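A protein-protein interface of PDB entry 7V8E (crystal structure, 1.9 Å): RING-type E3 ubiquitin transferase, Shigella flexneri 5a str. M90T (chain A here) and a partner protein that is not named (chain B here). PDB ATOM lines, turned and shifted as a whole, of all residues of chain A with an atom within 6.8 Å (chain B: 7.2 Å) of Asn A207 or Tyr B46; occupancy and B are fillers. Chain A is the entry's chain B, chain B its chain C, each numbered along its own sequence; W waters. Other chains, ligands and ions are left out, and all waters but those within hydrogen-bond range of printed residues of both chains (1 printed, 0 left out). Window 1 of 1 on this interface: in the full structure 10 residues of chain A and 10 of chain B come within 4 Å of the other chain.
Among the printed residues, merely in contact across the chains: Ala A164 with Leu B44 (3.8 Å), Arg A182 with Tyr B46 (3.5 Å), Val A184 with Asp B45 (3.2 Å), Val A184 with Tyr B46 (3.6 Å), Val A184 with Gly B47 (3.7 Å), Phe A205 with Tyr B46 (3.5 Å), Phe A205 with Phe B48 (3.6 Å), Asn A207 with Gly B47 (3.8 Å), Asn A207 with Phe B48 (3.8 Å), Phe A236 with Val B23 (3.8 Å), Phe A236 with Phe B48 (3.7 Å) and Phe A236 with Leu B84 (3.95 Å).
The backbone NH (N) of Asn A207 lies within hydrogen-bond range of the backbone carbonyl oxygen (O) of Ala A183 (2.9 Å). The backbone NH (N) of Met A186 lies within hydrogen-bond range of the backbone carbonyl oxygen (O) of Asn A207 (3.2 Å). The backbone carbonyl oxygen of Val A206 lies within hydrogen-bond range of the backbone NH of Phe A236 (2.8 Å). OD1 of Asn A207 lies within hydrogen-bond range of N of Ala A209 (3.1 Å). N of Val B15 lies within hydrogen-bond range of O of Val B23. N of Gly B47 lies within hydrogen-bond range of O of Val B42, 3.4 Å away.
Water W1 lies within hydrogen-bond range of O of Leu B44 (3.2 Å), OD1 of Asp B45 (3.2 Å) and NH1 of Arg A182 (3.2 Å).
Of the printed residues of chain A, Gly B47 touches Val A184 (3.7 Å), Met A186 (2.8 Å) and Asn A207 (3.8 Å). Of the printed residues of chain A, Phe B48 touches Phe A205 (3.6 Å), Asn A207 (3.8 Å) and Phe A236 (3.7 Å). The nearest residue of chain A that does not touch Tyr B46 is Met A186 (5.8 Å). The nearest printed residue of chain B that does not touch Met A186 is Phe B43 (4.5 Å).
O of Asp B45 is in hydrogen-bond range of NH1 of Arg A182 (2.7 Å). The backbone carbonyl oxygen (O) of Tyr B46 is in hydrogen-bond range of the side-chain amide nitrogen (ND2) of Asn A207, 2.9 Å away. SD of Met A186 sits close to O of Gly B47 (3.0 Å).
Printed residues of chain B that touch a printed residue of chain A: Val B23, Leu B44, Asp B45, Tyr B46, Gly B47, Phe B48 and Leu B84. Among the printed residues, 15 pairs touch across the chains. Among the printed residues, no Asp or Glu carboxylate lies within 4 Å of a Lys or Arg side-chain nitrogen of the other chain.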
ATOM      1  N   ALA A 164      -0.213   6.506  20.498  1.00  0.00           N
ATOM      2  CA  ALA A 164      -1.264   6.814  19.542  1.00  0.00           C
ATOM      3  C   ALA A 164      -0.598   7.451  18.337  1.00  0.00           C
ATOM      4  O   ALA A 164       0.061   8.493  18.462  1.00  0.00           O
ATOM      5  CB  ALA A 164      -2.338   7.727  20.139  1.00  0.00           C
ATOM      6  N   ASN A 181       0.343  -0.943  26.826  1.00  0.00           N
ATOM      7  CA  ASN A 181      -1.004  -1.413  27.079  1.00  0.00           C
ATOM      8  C   ASN A 181      -2.014  -0.884  26.081  1.00  0.00           C
ATOM      9  O   ASN A 181      -3.154  -1.355  26.077  1.00  0.00           O
ATOM     10  CB  ASN A 181      -1.461  -1.035  28.489  1.00  0.00           C
ATOM     11  CG  ASN A 181      -0.710  -1.794  29.556  1.00  0.00           C
ATOM     12  OD1 ASN A 181      -0.653  -3.029  29.542  1.00  0.00           O
ATOM     13  ND2 ASN A 181      -0.145  -1.055  30.511  1.00  0.00           N
ATOM     14  N   ARG A 182      -1.640   0.096  25.257  1.00  0.00           N
ATOM     15  CA  ARG A 182      -2.607   0.777  24.407  1.00  0.00           C
ATOM     16  C   ARG A 182      -1.862   1.298  23.191  1.00  0.00           C
ATOM     17  O   ARG A 182      -0.953   2.119  23.334  1.00  0.00           O
ATOM     18  CB  ARG A 182      -3.282   1.919  25.168  1.00  0.00           C
ATOM     19  CG  ARG A 182      -4.459   2.530  24.465  1.00  0.00           C
ATOM     20  CD  ARG A 182      -5.231   3.494  25.383  1.00  0.00           C
ATOM     21  NE  ARG A 182      -4.358   4.477  26.035  1.00  0.00           N
ATOM     22  CZ  ARG A 182      -3.775   5.506  25.422  1.00  0.00           C
ATOM     23  NH1 ARG A 182      -3.967   5.725  24.119  1.00  0.00           N
ATOM     24  NH2 ARG A 182      -3.002   6.335  26.123  1.00  0.00           N
ATOM     25  N   ALA A 183      -2.230   0.808  22.012  1.00  0.00           N
ATOM     26  CA  ALA A 183      -1.535   1.139  20.765  1.00  0.00           C
ATOM     27  C   ALA A 183      -2.576   1.454  19.710  1.00  0.00           C
ATOM     28  O   ALA A 183      -3.255   0.551  19.206  1.00  0.00           O
ATOM     29  CB  ALA A 183      -0.642  -0.010  20.303  1.00  0.00           C
ATOM     30  N   VAL A 184      -2.707   2.729  19.363  1.00  0.00           N
ATOM     31  CA  VAL A 184      -3.639   3.130  18.321  1.00  0.00           C
ATOM     32  C   VAL A 184      -2.811   3.269  17.049  1.00  0.00           C
ATOM     33  O   VAL A 184      -1.963   4.167  16.951  1.00  0.00           O
ATOM     34  CB  VAL A 184      -4.371   4.433  18.675  1.00  0.00           C
ATOM     35  CG1 VAL A 184      -5.393   4.784  17.607  1.00  0.00           C
ATOM     36  CG2 VAL A 184      -5.048   4.322  20.055  1.00  0.00           C
ATOM     37  N   LEU A 185      -3.002   2.341  16.105  1.00  0.00           N
ATOM     38  CA  LEU A 185      -2.226   2.311  14.861  1.00  0.00           C
ATOM     39  C   LEU A 185      -3.103   2.585  13.653  1.00  0.00           C
ATOM     40  O   LEU A 185      -2.642   2.464  12.508  1.00  0.00           O
ATOM     41  CB  LEU A 185      -1.533   0.951  14.693  1.00  0.00           C
ATOM     42  CG  LEU A 185      -0.808   0.399  15.921  1.00  0.00           C
ATOM     43  CD1 LEU A 185      -0.378  -1.024  15.660  1.00  0.00           C
ATOM     44  CD2 LEU A 185       0.411   1.244  16.238  1.00  0.00           C
ATOM     45  N   MET A 186      -4.348   2.968  13.892  1.00  0.00           N
ATOM     46  CA  MET A 186      -5.376   2.994  12.862  1.00  0.00           C
ATOM     47  C   MET A 186      -5.013   3.989  11.757  1.00  0.00           C
ATOM     48  O   MET A 186      -4.426   5.035  12.018  1.00  0.00           O
ATOM     49  CB  MET A 186      -6.694   3.393  13.513  1.00  0.00           C
ATOM     50  CG  MET A 186      -7.733   3.914  12.568  1.00  0.00           C
ATOM     51  SD  MET A 186      -9.230   4.251  13.486  1.00  0.00           S
ATOM     52  CE  MET A 186      -8.617   5.870  14.074  1.00  0.00           C
ATOM     53  N   ASN A 187      -5.418   3.690  10.518  1.00  0.00           N
ATOM     54  CA  ASN A 187      -5.282   4.639   9.399  1.00  0.00           C
ATOM     55  C   ASN A 187      -3.813   5.017   9.175  1.00  0.00           C
ATOM     56  O   ASN A 187      -3.409   6.166   9.339  1.00  0.00           O
ATOM     57  CB  ASN A 187      -6.119   5.905   9.624  1.00  0.00           C
ATOM     58  CG  ASN A 187      -7.591   5.683   9.433  1.00  0.00           C
ATOM     59  OD1 ASN A 187      -8.035   4.565   9.153  1.00  0.00           O
ATOM     60  ND2 ASN A 187      -8.370   6.755   9.590  1.00  0.00           N
ATOM     61  N   PHE A 205      -4.620  -3.319  24.478  1.00  0.00           N
ATOM     62  CA  PHE A 205      -5.490  -2.997  23.361  1.00  0.00           C
ATOM     63  C   PHE A 205      -4.674  -2.482  22.179  1.00  0.00           C
ATOM     64  O   PHE A 205      -3.789  -1.635  22.354  1.00  0.00           O
ATOM     65  CB  PHE A 205      -6.520  -1.941  23.739  1.00  0.00           C
ATOM     66  CG  PHE A 205      -7.332  -1.499  22.579  1.00  0.00           C
ATOM     67  CD1 PHE A 205      -8.176  -2.400  21.944  1.00  0.00           C
ATOM     68  CD2 PHE A 205      -7.221  -0.219  22.083  1.00  0.00           C
ATOM     69  CE1 PHE A 205      -8.917  -2.017  20.840  1.00  0.00           C
ATOM     70  CE2 PHE A 205      -7.954   0.172  20.999  1.00  0.00           C
ATOM     71  CZ  PHE A 205      -8.823  -0.721  20.381  1.00  0.00           C
ATOM     72  N   VAL A 206      -4.982  -2.985  20.985  1.00  0.00           N
ATOM     73  CA  VAL A 206      -4.337  -2.557  19.744  1.00  0.00           C
ATOM     74  C   VAL A 206      -5.407  -2.298  18.702  1.00  0.00           C
ATOM     75  O   VAL A 206      -6.246  -3.170  18.440  1.00  0.00           O
ATOM     76  CB  VAL A 206      -3.348  -3.606  19.202  1.00  0.00           C
ATOM     77  CG1 VAL A 206      -2.788  -3.146  17.854  1.00  0.00           C
ATOM     78  CG2 VAL A 206      -2.242  -3.856  20.194  1.00  0.00           C
ATOM     79  N   ASN A 207      -5.390  -1.100  18.106  1.00  0.00           N
ATOM     80  CA  ASN A 207      -6.337  -0.756  17.045  1.00  0.00           C
ATOM     81  C   ASN A 207      -5.525  -0.598  15.771  1.00  0.00           C
ATOM     82  O   ASN A 207      -4.684   0.300  15.682  1.00  0.00           O
ATOM     83  CB  ASN A 207      -7.111   0.519  17.379  1.00  0.00           C
ATOM     84  CG  ASN A 207      -8.145   0.881  16.318  1.00  0.00           C
ATOM     85  OD1 ASN A 207      -8.222   0.263  15.246  1.00  0.00           O
ATOM     86  ND2 ASN A 207      -8.935   1.915  16.606  1.00  0.00           N
ATOM     87  N   VAL A 208      -5.709  -1.517  14.823  1.00  0.00           N
ATOM     88  CA  VAL A 208      -4.927  -1.493  13.594  1.00  0.00           C
ATOM     89  C   VAL A 208      -5.836  -1.365  12.372  1.00  0.00           C
ATOM     90  O   VAL A 208      -5.439  -1.673  11.242  1.00  0.00           O
ATOM     91  CB  VAL A 208      -3.985  -2.714  13.518  1.00  0.00           C
ATOM     92  CG1 VAL A 208      -4.742  -4.010  13.175  1.00  0.00           C
ATOM     93  CG2 VAL A 208      -2.794  -2.434  12.607  1.00  0.00           C
ATOM     94  N   ALA A 209      -7.067  -0.909  12.596  1.00  0.00           N
ATOM     95  CA  ALA A 209      -8.025  -0.704  11.520  1.00  0.00           C
ATOM     96  C   ALA A 209      -7.493   0.302  10.505  1.00  0.00           C
ATOM     97  O   ALA A 209      -6.651   1.156  10.814  1.00  0.00           O
ATOM     98  CB  ALA A 209      -9.351  -0.218  12.091  1.00  0.00           C
ATOM     99  N   GLY A 210      -7.936   0.159   9.256  1.00  0.00           N
ATOM    100  CA  GLY A 210      -7.528   1.139   8.262  1.00  0.00           C
ATOM    101  C   GLY A 210      -6.082   1.071   7.833  1.00  0.00           C
ATOM    102  O   GLY A 210      -5.513   2.094   7.434  1.00  0.00           O
ATOM    103  N   ASN A 211      -5.445  -0.078   7.984  1.00  0.00           N
ATOM    104  CA  ASN A 211      -4.137  -0.393   7.438  1.00  0.00           C
ATOM    105  C   ASN A 211      -4.249  -1.467   6.369  1.00  0.00           C
ATOM    106  O   ASN A 211      -5.028  -2.415   6.536  1.00  0.00           O
ATOM    107  CB  ASN A 211      -3.193  -0.883   8.537  1.00  0.00           C
ATOM    108  CG  ASN A 211      -2.745   0.244   9.440  1.00  0.00           C
ATOM    109  OD1 ASN A 211      -1.750   0.907   9.163  1.00  0.00           O
ATOM    110  ND2 ASN A 211      -3.510   0.492  10.508  1.00  0.00           N
ATOM    111  N   ARG A 234      -6.218  -7.758  22.865  1.00  0.00           N
ATOM    112  CA  ARG A 234      -7.341  -7.582  21.956  1.00  0.00           C
ATOM    113  C   ARG A 234      -6.890  -6.711  20.790  1.00  0.00           C
ATOM    114  O   ARG A 234      -6.431  -5.577  20.995  1.00  0.00           O
ATOM    115  CB  ARG A 234      -8.523  -6.956  22.693  1.00  0.00           C
ATOM    116  CG  ARG A 234      -9.074  -7.843  23.822  1.00  0.00           C
ATOM    117  N   ILE A 235      -6.982  -7.240  19.575  1.00  0.00           N
ATOM    118  CA  ILE A 235      -6.578  -6.505  18.380  1.00  0.00           C
ATOM    119  C   ILE A 235      -7.816  -6.219  17.536  1.00  0.00           C
ATOM    120  O   ILE A 235      -8.516  -7.145  17.105  1.00  0.00           O
ATOM    121  CB  ILE A 235      -5.512  -7.263  17.577  1.00  0.00           C
ATOM    122  CG1 ILE A 235      -4.296  -7.546  18.458  1.00  0.00           C
ATOM    123  CG2 ILE A 235      -5.138  -6.473  16.339  1.00  0.00           C
ATOM    124  CD1 ILE A 235      -3.236  -8.404  17.782  1.00  0.00           C
ATOM    125  N   PHE A 236      -8.095  -4.939  17.310  1.00  0.00           N
ATOM    126  CA  PHE A 236      -9.168  -4.522  16.415  1.00  0.00           C
ATOM    127  C   PHE A 236      -8.600  -4.307  15.019  1.00  0.00           C
ATOM    128  O   PHE A 236      -7.719  -3.458  14.827  1.00  0.00           O
ATOM    129  CB  PHE A 236      -9.827  -3.232  16.901  1.00  0.00           C
ATOM    130  CG  PHE A 236     -10.920  -3.445  17.896  1.00  0.00           C
ATOM    131  CD1 PHE A 236     -11.062  -4.662  18.536  1.00  0.00           C
ATOM    132  CD2 PHE A 236     -11.806  -2.432  18.189  1.00  0.00           C
ATOM    133  CE1 PHE A 236     -12.067  -4.866  19.452  1.00  0.00           C
ATOM    134  CE2 PHE A 236     -12.815  -2.630  19.109  1.00  0.00           C
ATOM    135  CZ  PHE A 236     -12.941  -3.853  19.739  1.00  0.00           C
ATOM    136  N   PHE A 237      -9.102  -5.077  14.057  1.00  0.00           N
ATOM    137  CA  PHE A 237      -8.693  -5.019  12.659  1.00  0.00           C
ATOM    138  C   PHE A 237      -9.596  -4.168  11.781  1.00  0.00           C
ATOM    139  O   PHE A 237      -9.240  -3.918  10.622  1.00  0.00           O
ATOM    140  CB  PHE A 237      -8.664  -6.422  12.056  1.00  0.00           C
ATOM    141  CG  PHE A 237      -7.637  -7.320  12.653  1.00  0.00           C
ATOM    142  CD1 PHE A 237      -6.315  -7.243  12.247  1.00  0.00           C
ATOM    143  CD2 PHE A 237      -7.994  -8.256  13.610  1.00  0.00           C
ATOM    144  CE1 PHE A 237      -5.359  -8.087  12.795  1.00  0.00           C
ATOM    145  CE2 PHE A 237      -7.052  -9.104  14.162  1.00  0.00           C
ATOM    146  CZ  PHE A 237      -5.730  -9.024  13.752  1.00  0.00           C
ATOM    147  N   SER A 238     -10.775  -3.782  12.268  1.00  0.00           N
ATOM    148  CA  SER A 238     -11.752  -3.071  11.450  1.00  0.00           C
ATOM    149  C   SER A 238     -12.711  -2.249  12.311  1.00  0.00           C
ATOM    150  O   SER A 238     -13.196  -1.197  11.875  1.00  0.00           O
ATOM    151  CB  SER A 238     -12.541  -4.069  10.589  1.00  0.00           C
ATOM    152  OG  SER A 238     -13.510  -3.418   9.794  1.00  0.00           O
ATOM    153  N   VAL B  15     -16.565  -2.477  25.525  1.00  0.00           N
ATOM    154  CA  VAL B  15     -16.612  -2.070  24.130  1.00  0.00           C
ATOM    155  C   VAL B  15     -16.998  -3.269  23.283  1.00  0.00           C
ATOM    156  O   VAL B  15     -16.413  -4.348  23.433  1.00  0.00           O
ATOM    157  CB  VAL B  15     -15.266  -1.494  23.661  1.00  0.00           C
ATOM    158  CG1 VAL B  15     -15.418  -0.959  22.236  1.00  0.00           C
ATOM    159  CG2 VAL B  15     -14.784  -0.394  24.618  1.00  0.00           C
ATOM    160  N   VAL B  23     -13.784  -5.762  24.098  1.00  0.00           N
ATOM    161  CA  VAL B  23     -12.627  -5.370  24.895  1.00  0.00           C
ATOM    162  C   VAL B  23     -13.156  -4.529  26.051  1.00  0.00           C
ATOM    163  O   VAL B  23     -14.108  -3.754  25.894  1.00  0.00           O
ATOM    164  CB  VAL B  23     -11.578  -4.603  24.050  1.00  0.00           C
ATOM    165  CG1 VAL B  23     -12.196  -3.392  23.387  1.00  0.00           C
ATOM    166  CG2 VAL B  23     -10.383  -4.176  24.910  1.00  0.00           C
ATOM    167  N   THR B  24     -12.543  -4.684  27.215  1.00  0.00           N
ATOM    168  CA  THR B  24     -12.883  -3.880  28.379  1.00  0.00           C
ATOM    169  C   THR B  24     -11.777  -2.860  28.595  1.00  0.00           C
ATOM    170  O   THR B  24     -10.591  -3.198  28.545  1.00  0.00           O
ATOM    171  CB  THR B  24     -13.063  -4.745  29.624  1.00  0.00           C
ATOM    172  OG1 THR B  24     -14.252  -5.526  29.483  1.00  0.00           O
ATOM    173  CG2 THR B  24     -13.199  -3.861  30.851  1.00  0.00           C
ATOM    174  N   ILE B  25     -12.161  -1.606  28.771  1.00  0.00           N
ATOM    175  CA  ILE B  25     -11.199  -0.532  28.952  1.00  0.00           C
ATOM    176  C   ILE B  25     -11.573   0.217  30.223  1.00  0.00           C
ATOM    177  O   ILE B  25     -12.741   0.256  30.622  1.00  0.00           O
ATOM    178  CB  ILE B  25     -11.157   0.428  27.740  1.00  0.00           C
ATOM    179  CG1 ILE B  25     -12.468   1.192  27.608  1.00  0.00           C
ATOM    180  CG2 ILE B  25     -10.866  -0.315  26.452  1.00  0.00           C
ATOM    181  CD1 ILE B  25     -12.499   2.085  26.406  1.00  0.00           C
ATOM    182  N   TRP B  26     -10.566   0.806  30.865  1.00  0.00           N
ATOM    183  CA  TRP B  26     -10.758   1.623  32.055  1.00  0.00           C
ATOM    184  C   TRP B  26     -10.539   3.066  31.643  1.00  0.00           C
ATOM    185  O   TRP B  26      -9.447   3.419  31.199  1.00  0.00           O
ATOM    186  CB  TRP B  26      -9.759   1.266  33.161  1.00  0.00           C
ATOM    187  CG  TRP B  26      -9.820  -0.137  33.668  1.00  0.00           C
ATOM    188  CD1 TRP B  26      -8.920  -1.141  33.426  1.00  0.00           C
ATOM    189  CD2 TRP B  26     -10.806  -0.683  34.544  1.00  0.00           C
ATOM    190  NE1 TRP B  26      -9.299  -2.281  34.087  1.00  0.00           N
ATOM    191  CE2 TRP B  26     -10.457  -2.031  34.778  1.00  0.00           C
ATOM    192  CE3 TRP B  26     -11.955  -0.167  35.148  1.00  0.00           C
ATOM    193  CZ2 TRP B  26     -11.223  -2.872  35.592  1.00  0.00           C
ATOM    194  CZ3 TRP B  26     -12.713  -0.999  35.955  1.00  0.00           C
ATOM    195  CH2 TRP B  26     -12.349  -2.341  36.163  1.00  0.00           C
ATOM    196  N   LEU B  27     -11.539   3.901  31.855  1.00  0.00           N
ATOM    197  CA  LEU B  27     -11.434   5.319  31.561  1.00  0.00           C
ATOM    198  C   LEU B  27     -11.443   6.101  32.862  1.00  0.00           C
ATOM    199  O   LEU B  27     -11.920   5.616  33.891  1.00  0.00           O
ATOM    200  CB  LEU B  27     -12.588   5.798  30.678  1.00  0.00           C
ATOM    201  CG  LEU B  27     -12.767   5.176  29.294  1.00  0.00           C
ATOM    202  CD1 LEU B  27     -13.861   5.957  28.583  1.00  0.00           C
ATOM    203  CD2 LEU B  27     -11.474   5.214  28.495  1.00  0.00           C
ATOM    204  N   ASP B  40     -14.732  12.363  22.235  1.00  0.00           N
ATOM    205  CA  ASP B  40     -13.461  12.927  21.800  1.00  0.00           C
ATOM    206  C   ASP B  40     -12.295  12.281  22.531  1.00  0.00           C
ATOM    207  O   ASP B  40     -11.257  11.977  21.924  1.00  0.00           O
ATOM    208  CB  ASP B  40     -13.467  14.440  22.034  1.00  0.00           C
ATOM    209  N   MET B  41     -12.434  12.077  23.842  1.00  0.00           N
ATOM    210  CA  MET B  41     -11.364  11.437  24.595  1.00  0.00           C
ATOM    211  C   MET B  41     -11.086  10.043  24.068  1.00  0.00           C
ATOM    212  O   MET B  41      -9.926   9.623  23.959  1.00  0.00           O
ATOM    213  CB  MET B  41     -11.736  11.338  26.068  1.00  0.00           C
ATOM    214  CG  MET B  41     -10.563  10.923  26.950  1.00  0.00           C
ATOM    215  SD  MET B  41     -10.985  10.863  28.698  1.00  0.00           S
ATOM    216  CE  MET B  41     -12.337   9.717  28.674  1.00  0.00           C
ATOM    217  N   VAL B  42     -12.144   9.297  23.778  1.00  0.00           N
ATOM    218  CA  VAL B  42     -11.972   7.916  23.331  1.00  0.00           C
ATOM    219  C   VAL B  42     -11.433   7.873  21.902  1.00  0.00           C
ATOM    220  O   VAL B  42     -10.665   6.967  21.553  1.00  0.00           O
ATOM    221  CB  VAL B  42     -13.313   7.178  23.507  1.00  0.00           C
ATOM    222  CG1 VAL B  42     -13.332   5.819  22.781  1.00  0.00           C
ATOM    223  CG2 VAL B  42     -13.564   6.993  25.009  1.00  0.00           C
ATOM    224  N   PHE B  43     -11.821   8.845  21.061  1.00  0.00           N
ATOM    225  CA  PHE B  43     -11.243   8.981  19.719  1.00  0.00           C
ATOM    226  C   PHE B  43      -9.724   9.074  19.775  1.00  0.00           C
ATOM    227  O   PHE B  43      -9.017   8.356  19.056  1.00  0.00           O
ATOM    228  CB  PHE B  43     -11.811  10.221  19.019  1.00  0.00           C
ATOM    229  CG  PHE B  43     -11.268  10.449  17.612  1.00  0.00           C
ATOM    230  CD1 PHE B  43     -11.270   9.428  16.669  1.00  0.00           C
ATOM    231  CD2 PHE B  43     -10.741  11.683  17.248  1.00  0.00           C
ATOM    232  CE1 PHE B  43     -10.767   9.631  15.386  1.00  0.00           C
ATOM    233  CE2 PHE B  43     -10.229  11.892  15.956  1.00  0.00           C
ATOM    234  CZ  PHE B  43     -10.250  10.860  15.031  1.00  0.00           C
ATOM    235  N   LEU B  44      -9.202   9.958  20.619  1.00  0.00           N
ATOM    236  CA  LEU B  44      -7.753  10.134  20.697  1.00  0.00           C
ATOM    237  C   LEU B  44      -7.065   8.932  21.341  1.00  0.00           C
ATOM    238  O   LEU B  44      -6.002   8.501  20.873  1.00  0.00           O
ATOM    239  CB  LEU B  44      -7.422  11.413  21.467  1.00  0.00           C
ATOM    240  CG  LEU B  44      -5.971  11.908  21.466  1.00  0.00           C
ATOM    241  CD1 LEU B  44      -5.311  11.765  20.095  1.00  0.00           C
ATOM    242  CD2 LEU B  44      -5.907  13.358  21.930  1.00  0.00           C
ATOM    243  N   ASP B  45      -7.659   8.362  22.406  1.00  0.00           N
ATOM    244  CA  ASP B  45      -6.979   7.325  23.183  1.00  0.00           C
ATOM    245  C   ASP B  45      -7.133   5.924  22.602  1.00  0.00           C
ATOM    246  O   ASP B  45      -6.323   5.055  22.932  1.00  0.00           O
ATOM    247  CB  ASP B  45      -7.496   7.280  24.634  1.00  0.00           C
ATOM    248  CG  ASP B  45      -7.046   8.457  25.477  1.00  0.00           C
ATOM    249  OD1 ASP B  45      -6.291   9.316  24.975  1.00  0.00           O
ATOM    250  OD2 ASP B  45      -7.440   8.499  26.672  1.00  0.00           O
ATOM    251  N   TYR B  46      -8.169   5.676  21.791  1.00  0.00           N
ATOM    252  CA  TYR B  46      -8.476   4.337  21.273  1.00  0.00           C
ATOM    253  C   TYR B  46      -8.678   4.297  19.766  1.00  0.00           C
ATOM    254  O   TYR B  46      -8.690   3.204  19.181  1.00  0.00           O
ATOM    255  CB  TYR B  46      -9.720   3.771  21.986  1.00  0.00           C
ATOM    256  CG  TYR B  46      -9.374   3.523  23.424  1.00  0.00           C
ATOM    257  CD1 TYR B  46      -8.790   2.332  23.808  1.00  0.00           C
ATOM    258  CD2 TYR B  46      -9.553   4.508  24.386  1.00  0.00           C
ATOM    259  CE1 TYR B  46      -8.430   2.109  25.130  1.00  0.00           C
ATOM    260  CE2 TYR B  46      -9.177   4.296  25.696  1.00  0.00           C
ATOM    261  CZ  TYR B  46      -8.617   3.099  26.057  1.00  0.00           C
ATOM    262  OH  TYR B  46      -8.273   2.880  27.370  1.00  0.00           O
ATOM    263  N   GLY B  47      -8.839   5.447  19.128  1.00  0.00           N
ATOM    264  CA  GLY B  47      -8.998   5.520  17.696  1.00  0.00           C
ATOM    265  C   GLY B  47     -10.413   5.376  17.193  1.00  0.00           C
ATOM    266  O   GLY B  47     -10.602   5.275  15.986  1.00  0.00           O
ATOM    267  N   PHE B  48     -11.415   5.327  18.062  1.00  0.00           N
ATOM    268  CA  PHE B  48     -12.788   5.151  17.576  1.00  0.00           C
ATOM    269  C   PHE B  48     -13.392   6.494  17.165  1.00  0.00           C
ATOM    270  O   PHE B  48     -13.553   7.381  18.020  1.00  0.00           O
ATOM    271  CB  PHE B  48     -13.661   4.481  18.633  1.00  0.00           C
ATOM    272  CG  PHE B  48     -13.068   3.218  19.220  1.00  0.00           C
ATOM    273  CD1 PHE B  48     -12.312   2.358  18.441  1.00  0.00           C
ATOM    274  CD2 PHE B  48     -13.287   2.888  20.552  1.00  0.00           C
ATOM    275  CE1 PHE B  48     -11.771   1.204  18.995  1.00  0.00           C
ATOM    276  CE2 PHE B  48     -12.770   1.735  21.096  1.00  0.00           C
ATOM    277  CZ  PHE B  48     -12.023   0.888  20.326  1.00  0.00           C
ATOM    278  N   PRO B  49     -13.763   6.681  15.899  1.00  0.00           N
ATOM    279  CA  PRO B  49     -14.321   7.976  15.463  1.00  0.00           C
ATOM    280  C   PRO B  49     -15.613   8.284  16.200  1.00  0.00           C
ATOM    281  O   PRO B  49     -16.459   7.395  16.393  1.00  0.00           O
ATOM    282  CB  PRO B  49     -14.569   7.774  13.957  1.00  0.00           C
ATOM    283  CG  PRO B  49     -13.653   6.631  13.568  1.00  0.00           C
ATOM    284  CD  PRO B  49     -13.601   5.737  14.779  1.00  0.00           C
ATOM    285  N   LEU B  82     -20.105   0.678  25.304  1.00  0.00           N
ATOM    286  CA  LEU B  82     -19.786   1.378  24.069  1.00  0.00           C
ATOM    287  C   LEU B  82     -19.927   0.406  22.905  1.00  0.00           C
ATOM    288  O   LEU B  82     -19.256  -0.632  22.881  1.00  0.00           O
ATOM    289  CB  LEU B  82     -18.354   1.929  24.125  1.00  0.00           C
ATOM    290  CG  LEU B  82     -17.756   2.536  22.841  1.00  0.00           C
ATOM    291  CD1 LEU B  82     -18.572   3.764  22.398  1.00  0.00           C
ATOM    292  CD2 LEU B  82     -16.319   2.969  23.058  1.00  0.00           C
ATOM    293  N   LEU B  84     -19.702   0.072  18.655  1.00  0.00           N
ATOM    294  CA  LEU B  84     -19.075   0.733  17.512  1.00  0.00           C
ATOM    295  C   LEU B  84     -19.814   0.406  16.214  1.00  0.00           C
ATOM    296  O   LEU B  84     -19.958  -0.765  15.844  1.00  0.00           O
ATOM    297  CB  LEU B  84     -17.591   0.367  17.409  1.00  0.00           C
ATOM    298  CG  LEU B  84     -16.727   0.785  18.603  1.00  0.00           C
ATOM    299  CD1 LEU B  84     -15.280   0.378  18.394  1.00  0.00           C
ATOM    300  CD2 LEU B  84     -16.815   2.317  18.823  1.00  0.00           C
HETATM  301  O   HOH W   1      -3.755   8.775  23.080  1.00  0.00           O
